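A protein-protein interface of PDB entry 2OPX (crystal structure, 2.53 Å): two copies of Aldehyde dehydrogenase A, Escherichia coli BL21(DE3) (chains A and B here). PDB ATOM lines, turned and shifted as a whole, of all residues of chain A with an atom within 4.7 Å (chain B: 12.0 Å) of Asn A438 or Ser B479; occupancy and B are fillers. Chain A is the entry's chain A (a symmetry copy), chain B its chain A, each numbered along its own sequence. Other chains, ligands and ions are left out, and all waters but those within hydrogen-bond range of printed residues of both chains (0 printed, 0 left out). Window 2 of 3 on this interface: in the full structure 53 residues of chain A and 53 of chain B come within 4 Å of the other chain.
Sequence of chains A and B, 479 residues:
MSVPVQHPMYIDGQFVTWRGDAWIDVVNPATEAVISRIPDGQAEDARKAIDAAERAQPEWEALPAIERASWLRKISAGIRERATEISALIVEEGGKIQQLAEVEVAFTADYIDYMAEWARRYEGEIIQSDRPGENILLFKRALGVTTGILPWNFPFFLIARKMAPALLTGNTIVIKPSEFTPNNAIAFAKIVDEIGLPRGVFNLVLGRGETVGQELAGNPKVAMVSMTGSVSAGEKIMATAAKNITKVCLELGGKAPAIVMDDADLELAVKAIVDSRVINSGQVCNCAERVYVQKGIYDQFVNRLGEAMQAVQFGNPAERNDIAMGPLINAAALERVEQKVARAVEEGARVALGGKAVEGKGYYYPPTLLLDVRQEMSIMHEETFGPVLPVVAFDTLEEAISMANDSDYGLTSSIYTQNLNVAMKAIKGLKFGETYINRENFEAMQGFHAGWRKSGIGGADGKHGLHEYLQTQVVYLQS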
ATOM      1  N   LEU A 268      13.693  36.711  -5.814  1.00  0.00           N
ATOM      2  CA  LEU A 268      14.513  35.754  -5.085  1.00  0.00           C
ATOM      3  C   LEU A 268      15.623  36.463  -4.319  1.00  0.00           C
ATOM      4  O   LEU A 268      15.853  36.198  -3.136  1.00  0.00           O
ATOM      5  CB  LEU A 268      15.132  34.746  -6.052  1.00  0.00           C
ATOM      6  CG  LEU A 268      16.036  33.696  -5.402  1.00  0.00           C
ATOM      7  CD1 LEU A 268      15.200  32.815  -4.491  1.00  0.00           C
ATOM      8  CD2 LEU A 268      16.709  32.854  -6.465  1.00  0.00           C
ATOM      9  N   ILE A 415      25.719  35.951  -4.352  1.00  0.00           N
ATOM     10  CA  ILE A 415      25.524  36.581  -5.643  1.00  0.00           C
ATOM     11  C   ILE A 415      24.304  35.975  -6.292  1.00  0.00           C
ATOM     12  O   ILE A 415      24.057  34.770  -6.182  1.00  0.00           O
ATOM     13  CB  ILE A 415      26.742  36.386  -6.570  1.00  0.00           C
ATOM     14  CG1 ILE A 415      26.484  37.087  -7.908  1.00  0.00           C
ATOM     15  CG2 ILE A 415      27.018  34.901  -6.768  1.00  0.00           C
ATOM     16  CD1 ILE A 415      27.667  37.089  -8.857  1.00  0.00           C
ATOM     17  N   TYR A 416      23.527  36.823  -6.956  1.00  0.00           N
ATOM     18  CA  TYR A 416      22.324  36.367  -7.626  1.00  0.00           C
ATOM     19  C   TYR A 416      22.454  36.668  -9.101  1.00  0.00           C
ATOM     20  O   TYR A 416      22.626  37.819  -9.514  1.00  0.00           O
ATOM     21  CB  TYR A 416      21.106  37.049  -7.013  1.00  0.00           C
ATOM     22  CG  TYR A 416      21.114  36.908  -5.512  1.00  0.00           C
ATOM     23  CD1 TYR A 416      21.935  37.715  -4.728  1.00  0.00           C
ATOM     24  CD2 TYR A 416      20.380  35.902  -4.880  1.00  0.00           C
ATOM     25  CE1 TYR A 416      22.035  37.528  -3.356  1.00  0.00           C
ATOM     26  CE2 TYR A 416      20.474  35.704  -3.501  1.00  0.00           C
ATOM     27  CZ  TYR A 416      21.308  36.524  -2.752  1.00  0.00           C
ATOM     28  OH  TYR A 416      21.434  36.332  -1.401  1.00  0.00           O
ATOM     29  N   THR A 417      22.398  35.610  -9.893  1.00  0.00           N
ATOM     30  CA  THR A 417      22.531  35.737 -11.326  1.00  0.00           C
ATOM     31  C   THR A 417      21.949  34.484 -11.960  1.00  0.00           C
ATOM     32  O   THR A 417      21.622  33.520 -11.263  1.00  0.00           O
ATOM     33  CB  THR A 417      24.026  35.896 -11.712  1.00  0.00           C
ATOM     34  OG1 THR A 417      24.141  36.168 -13.110  1.00  0.00           O
ATOM     35  CG2 THR A 417      24.804  34.628 -11.382  1.00  0.00           C
ATOM     36  N   TYR A 436      27.112  31.966  -1.470  1.00  0.00           N
ATOM     37  CA  TYR A 436      25.778  31.463  -1.738  1.00  0.00           C
ATOM     38  C   TYR A 436      25.358  32.006  -3.094  1.00  0.00           C
ATOM     39  O   TYR A 436      25.593  33.175  -3.410  1.00  0.00           O
ATOM     40  CB  TYR A 436      24.816  31.934  -0.658  1.00  0.00           C
ATOM     41  CG  TYR A 436      25.110  31.325   0.682  1.00  0.00           C
ATOM     42  CD1 TYR A 436      24.588  30.077   1.032  1.00  0.00           C
ATOM     43  CD2 TYR A 436      25.944  31.977   1.593  1.00  0.00           C
ATOM     44  CE1 TYR A 436      24.888  29.496   2.260  1.00  0.00           C
ATOM     45  CE2 TYR A 436      26.255  31.403   2.818  1.00  0.00           C
ATOM     46  CZ  TYR A 436      25.725  30.165   3.144  1.00  0.00           C
ATOM     47  OH  TYR A 436      26.049  29.593   4.347  1.00  0.00           O
ATOM     48  N   ILE A 437      24.748  31.148  -3.898  1.00  0.00           N
ATOM     49  CA  ILE A 437      24.310  31.545  -5.220  1.00  0.00           C
ATOM     50  C   ILE A 437      22.821  31.295  -5.381  1.00  0.00           C
ATOM     51  O   ILE A 437      22.379  30.149  -5.460  1.00  0.00           O
ATOM     52  CB  ILE A 437      25.095  30.786  -6.291  1.00  0.00           C
ATOM     53  CG1 ILE A 437      26.568  31.183  -6.199  1.00  0.00           C
ATOM     54  CG2 ILE A 437      24.541  31.091  -7.671  1.00  0.00           C
ATOM     55  CD1 ILE A 437      27.459  30.429  -7.147  1.00  0.00           C
ATOM     56  N   ASN A 438      22.061  32.388  -5.406  1.00  0.00           N
ATOM     57  CA  ASN A 438      20.612  32.355  -5.560  1.00  0.00           C
ATOM     58  C   ASN A 438      19.876  31.740  -4.380  1.00  0.00           C
ATOM     59  O   ASN A 438      18.931  30.972  -4.559  1.00  0.00           O
ATOM     60  CB  ASN A 438      20.242  31.623  -6.846  1.00  0.00           C
ATOM     61  CG  ASN A 438      20.763  32.328  -8.078  1.00  0.00           C
ATOM     62  OD1 ASN A 438      20.942  31.708  -9.126  1.00  0.00           O
ATOM     63  ND2 ASN A 438      20.998  33.633  -7.967  1.00  0.00           N
ATOM     64  N   ARG A 439      20.317  32.085  -3.175  1.00  0.00           N
ATOM     65  CA  ARG A 439      19.689  31.613  -1.942  1.00  0.00           C
ATOM     66  C   ARG A 439      20.273  32.360  -0.752  1.00  0.00           C
ATOM     67  O   ARG A 439      21.314  33.006  -0.876  1.00  0.00           O
ATOM     68  CB  ARG A 439      19.879  30.107  -1.755  1.00  0.00           C
ATOM     69  CG  ARG A 439      21.314  29.644  -1.730  1.00  0.00           C
ATOM     70  CD  ARG A 439      21.437  28.381  -0.889  1.00  0.00           C
ATOM     71  NE  ARG A 439      21.419  28.694   0.538  1.00  0.00           N
ATOM     72  CZ  ARG A 439      21.594  27.806   1.510  1.00  0.00           C
ATOM     73  NH1 ARG A 439      21.797  26.528   1.224  1.00  0.00           N
ATOM     74  NH2 ARG A 439      21.587  28.205   2.775  1.00  0.00           N
ATOM     75  N   SER B 129      23.641  17.937  -0.347  1.00  0.00           N
ATOM     76  CA  SER B 129      22.881  18.955   0.352  1.00  0.00           C
ATOM     77  C   SER B 129      21.526  18.408   0.751  1.00  0.00           C
ATOM     78  O   SER B 129      21.029  17.469   0.132  1.00  0.00           O
ATOM     79  CB  SER B 129      22.686  20.171  -0.556  1.00  0.00           C
ATOM     80  OG  SER B 129      21.714  21.057  -0.027  1.00  0.00           O
ATOM     81  N   ARG B 131      19.019  20.336   0.669  1.00  0.00           N
ATOM     82  CA  ARG B 131      18.141  21.125  -0.173  1.00  0.00           C
ATOM     83  C   ARG B 131      18.075  20.561  -1.574  1.00  0.00           C
ATOM     84  O   ARG B 131      19.101  20.293  -2.192  1.00  0.00           O
ATOM     85  CB  ARG B 131      18.621  22.571  -0.245  1.00  0.00           C
ATOM     86  CG  ARG B 131      18.674  23.250   1.096  1.00  0.00           C
ATOM     87  CD  ARG B 131      18.741  24.750   0.946  1.00  0.00           C
ATOM     88  NE  ARG B 131      18.744  25.397   2.249  1.00  0.00           N
ATOM     89  CZ  ARG B 131      18.493  26.684   2.442  1.00  0.00           C
ATOM     90  NH1 ARG B 131      18.213  27.467   1.407  1.00  0.00           N
ATOM     91  NH2 ARG B 131      18.528  27.187   3.671  1.00  0.00           N
ATOM     92  N   PRO B 132      16.856  20.359  -2.091  1.00  0.00           N
ATOM     93  CA  PRO B 132      16.683  19.821  -3.439  1.00  0.00           C
ATOM     94  C   PRO B 132      17.220  20.815  -4.456  1.00  0.00           C
ATOM     95  O   PRO B 132      17.069  22.025  -4.290  1.00  0.00           O
ATOM     96  CB  PRO B 132      15.169  19.657  -3.556  1.00  0.00           C
ATOM     97  CG  PRO B 132      14.732  19.451  -2.139  1.00  0.00           C
ATOM     98  CD  PRO B 132      15.562  20.458  -1.395  1.00  0.00           C
ATOM     99  N   GLY B 133      17.861  20.299  -5.498  1.00  0.00           N
ATOM    100  CA  GLY B 133      18.388  21.163  -6.537  1.00  0.00           C
ATOM    101  C   GLY B 133      19.595  21.990  -6.146  1.00  0.00           C
ATOM    102  O   GLY B 133      20.021  22.869  -6.901  1.00  0.00           O
ATOM    103  N   GLU B 134      20.152  21.730  -4.968  1.00  0.00           N
ATOM    104  CA  GLU B 134      21.323  22.475  -4.543  1.00  0.00           C
ATOM    105  C   GLU B 134      22.598  21.647  -4.664  1.00  0.00           C
ATOM    106  O   GLU B 134      22.600  20.432  -4.464  1.00  0.00           O
ATOM    107  CB  GLU B 134      21.168  22.965  -3.101  1.00  0.00           C
ATOM    108  CG  GLU B 134      22.343  23.815  -2.636  1.00  0.00           C
ATOM    109  CD  GLU B 134      22.197  24.318  -1.213  1.00  0.00           C
ATOM    110  OE1 GLU B 134      22.136  23.490  -0.283  1.00  0.00           O
ATOM    111  OE2 GLU B 134      22.146  25.548  -1.023  1.00  0.00           O
ATOM    112  N   ASN B 135      23.682  22.320  -5.017  1.00  0.00           N
ATOM    113  CA  ASN B 135      24.975  21.676  -5.133  1.00  0.00           C
ATOM    114  C   ASN B 135      25.927  22.360  -4.162  1.00  0.00           C
ATOM    115  O   ASN B 135      26.044  23.582  -4.154  1.00  0.00           O
ATOM    116  CB  ASN B 135      25.510  21.805  -6.560  1.00  0.00           C
ATOM    117  CG  ASN B 135      25.054  20.675  -7.462  1.00  0.00           C
ATOM    118  OD1 ASN B 135      24.940  20.844  -8.674  1.00  0.00           O
ATOM    119  ND2 ASN B 135      24.809  19.509  -6.878  1.00  0.00           N
ATOM    120  N   ILE B 136      26.586  21.583  -3.316  1.00  0.00           N
ATOM    121  CA  ILE B 136      27.536  22.177  -2.394  1.00  0.00           C
ATOM    122  C   ILE B 136      28.928  21.852  -2.907  1.00  0.00           C
ATOM    123  O   ILE B 136      29.379  20.706  -2.849  1.00  0.00           O
ATOM    124  CB  ILE B 136      27.373  21.640  -0.972  1.00  0.00           C
ATOM    125  CG1 ILE B 136      25.971  21.979  -0.455  1.00  0.00           C
ATOM    126  CG2 ILE B 136      28.433  22.257  -0.068  1.00  0.00           C
ATOM    127  CD1 ILE B 136      25.656  21.415   0.924  1.00  0.00           C
ATOM    128  N   LEU B 137      29.592  22.877  -3.431  1.00  0.00           N
ATOM    129  CA  LEU B 137      30.927  22.724  -3.979  1.00  0.00           C
ATOM    130  C   LEU B 137      31.946  23.357  -3.055  1.00  0.00           C
ATOM    131  O   LEU B 137      31.909  24.564  -2.813  1.00  0.00           O
ATOM    132  CB  LEU B 137      31.008  23.392  -5.351  1.00  0.00           C
ATOM    133  CG  LEU B 137      29.839  23.118  -6.300  1.00  0.00           C
ATOM    134  CD1 LEU B 137      30.019  23.947  -7.569  1.00  0.00           C
ATOM    135  CD2 LEU B 137      29.762  21.636  -6.619  1.00  0.00           C
ATOM    136  N   VAL B 474      33.353  27.215   0.303  1.00  0.00           N
ATOM    137  CA  VAL B 474      32.176  26.382   0.140  1.00  0.00           C
ATOM    138  C   VAL B 474      31.135  27.156  -0.655  1.00  0.00           C
ATOM    139  O   VAL B 474      30.661  28.207  -0.223  1.00  0.00           O
ATOM    140  CB  VAL B 474      31.591  25.984   1.508  1.00  0.00           C
ATOM    141  CG1 VAL B 474      30.311  25.183   1.320  1.00  0.00           C
ATOM    142  CG2 VAL B 474      32.624  25.179   2.283  1.00  0.00           C
ATOM    143  N   VAL B 475      30.799  26.642  -1.830  1.00  0.00           N
ATOM    144  CA  VAL B 475      29.815  27.290  -2.680  1.00  0.00           C
ATOM    145  C   VAL B 475      28.475  26.564  -2.614  1.00  0.00           C
ATOM    146  O   VAL B 475      28.396  25.363  -2.872  1.00  0.00           O
ATOM    147  CB  VAL B 475      30.289  27.334  -4.162  1.00  0.00           C
ATOM    148  CG1 VAL B 475      29.236  28.001  -5.032  1.00  0.00           C
ATOM    149  CG2 VAL B 475      31.608  28.088  -4.267  1.00  0.00           C
ATOM    150  N   TYR B 476      27.429  27.297  -2.245  1.00  0.00           N
ATOM    151  CA  TYR B 476      26.088  26.733  -2.189  1.00  0.00           C
ATOM    152  C   TYR B 476      25.371  27.200  -3.451  1.00  0.00           C
ATOM    153  O   TYR B 476      24.816  28.295  -3.490  1.00  0.00           O
ATOM    154  CB  TYR B 476      25.330  27.229  -0.960  1.00  0.00           C
ATOM    155  CG  TYR B 476      25.856  26.709   0.350  1.00  0.00           C
ATOM    156  CD1 TYR B 476      26.954  27.305   0.966  1.00  0.00           C
ATOM    157  CD2 TYR B 476      25.245  25.626   0.987  1.00  0.00           C
ATOM    158  CE1 TYR B 476      27.431  26.842   2.189  1.00  0.00           C
ATOM    159  CE2 TYR B 476      25.715  25.152   2.207  1.00  0.00           C
ATOM    160  CZ  TYR B 476      26.808  25.767   2.803  1.00  0.00           C
ATOM    161  OH  TYR B 476      27.273  25.319   4.014  1.00  0.00           O
ATOM    162  N   LEU B 477      25.396  26.364  -4.483  1.00  0.00           N
ATOM    163  CA  LEU B 477      24.778  26.688  -5.761  1.00  0.00           C
ATOM    164  C   LEU B 477      23.329  26.211  -5.855  1.00  0.00           C
ATOM    165  O   LEU B 477      23.058  25.023  -5.717  1.00  0.00           O
ATOM    166  CB  LEU B 477      25.595  26.051  -6.886  1.00  0.00           C
ATOM    167  CG  LEU B 477      25.836  26.872  -8.149  1.00  0.00           C
ATOM    168  CD1 LEU B 477      26.498  25.992  -9.194  1.00  0.00           C
ATOM    169  CD2 LEU B 477      24.524  27.414  -8.670  1.00  0.00           C
ATOM    170  N   GLN B 478      22.408  27.142  -6.098  1.00  0.00           N
ATOM    171  CA  GLN B 478      20.986  26.822  -6.234  1.00  0.00           C
ATOM    172  C   GLN B 478      20.517  26.938  -7.688  1.00  0.00           C
ATOM    173  O   GLN B 478      19.821  26.050  -8.199  1.00  0.00           O
ATOM    174  CB  GLN B 478      20.147  27.753  -5.363  1.00  0.00           C
ATOM    175  CG  GLN B 478      20.138  27.406  -3.885  1.00  0.00           C
ATOM    176  CD  GLN B 478      19.192  26.262  -3.544  1.00  0.00           C
ATOM    177  OE1 GLN B 478      18.977  25.954  -2.369  1.00  0.00           O
ATOM    178  NE2 GLN B 478      18.625  25.626  -4.567  1.00  0.00           N
ATOM    179  N   SER B 479      20.905  28.036  -8.337  1.00  0.00           N
ATOM    180  CA  SER B 479      20.559  28.327  -9.737  1.00  0.00           C
ATOM    181  C   SER B 479      19.057  28.402 -10.024  1.00  0.00           C
ATOM    182  O   SER B 479      18.643  27.911 -11.099  1.00  0.00           O
ATOM    183  CB  SER B 479      21.188  27.289 -10.683  1.00  0.00           C
ATOM    184  OG  SER B 479      20.505  26.043 -10.636  1.00  0.00           O
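The side-chain carboxylate (OE1) of Glu B134 sits at hydrogen-bond distance from the side-chain hydroxyl (OG) of Ser B129, at 2.5 Å.
OE2 of Glu B134 sits close to OE1 of Gln B478 (3.5 Å).
N of Asn B135 sits at hydrogen-bond distance from O of Leu B477, at 2.9 Å.
The backbone carbonyl oxygen of Leu B137 is in hydrogen-bond range of the backbone NH of Val B475, 2.6 Å away.
The backbone NH of Asn A438 is in hydrogen-bond range of the backbone carbonyl oxygen of Ile A415 (3.2 Å).
O of Thr A417 sits close to OD1 of Asn A438.
No position is printed for both chains.
Of the 12 pairs that touch across the chains among the printed residues, none has its exchanged pair printed and touching as well.
Asn A438 touches two residues of chain B.
Of chain A, only Ile A437 and Asn A438 come within 4 Å of Ser B479.
No residue of chain B comes within 4 Å of Leu A268.
No residue of chain B comes within 4 Å of Ile A415.
No residue of chain B comes within 4 Å of Tyr A416.
Ile A437 touches just these residues of chain B: Val B475 (3.7 Å), Tyr B476 (2.9 Å), Leu B477 (3.8 Å), Gln B478 (3.1 Å) and Ser B479 (3.9 Å).
Of the printed residues of chain A, Tyr B476 touches Tyr A436, Ile A437 and Arg A439.
Printed residues of chain A within 4 Å of Glu B134: Arg A439 (2.5 Å).
Asn B135 touches none of the printed residues of chain A.
Leu B137 touches none of the printed residues of chain A.
The nearest residue of chain B that does not touch Asn A438 is Tyr B476 (5.3 Å).
The side-chain carboxylate (OE2) of Glu B134 lies within salt-bridge range of the guanidinium group (NH1) of Arg A439 (2.5 Å).
The backbone carbonyl oxygen (O) of Tyr B476 sits at hydrogen-bond distance from the backbone NH (N) of Ile A437 (2.9 Å).
N of Gln B478 sits at hydrogen-bond distance from O of Ile A437 (3.1 Å).
The guanidinium group (NH2) of Arg A439 sits close to the guanidinium group (NH2) of Arg B131 (3.3 Å).
Printed residues of chain A that touch a printed residue of chain B: Tyr A436, Ile A437, Asn A438 and Arg A439.
Hydrophobic or aromatic side chains of chain A within 4 Å of the printed part of chain B: Tyr A436 and Ile A437.
Among the printed residues, Asp or Glu carboxylates within 4 Å of a Lys or Arg side-chain nitrogen of the other chain: Arg A439 with Glu B134.
Among the printed residues, merely in contact across the chains: Tyr A436 with Tyr B476, Arg A439 with Gln B478, Asn A438 with Ser B479, Asn A438 with Gln B478, Arg A439 with Tyr B476, Ile A437 with Val B475, Ile A437 with Leu B477 and Ile A437 with Ser B479.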
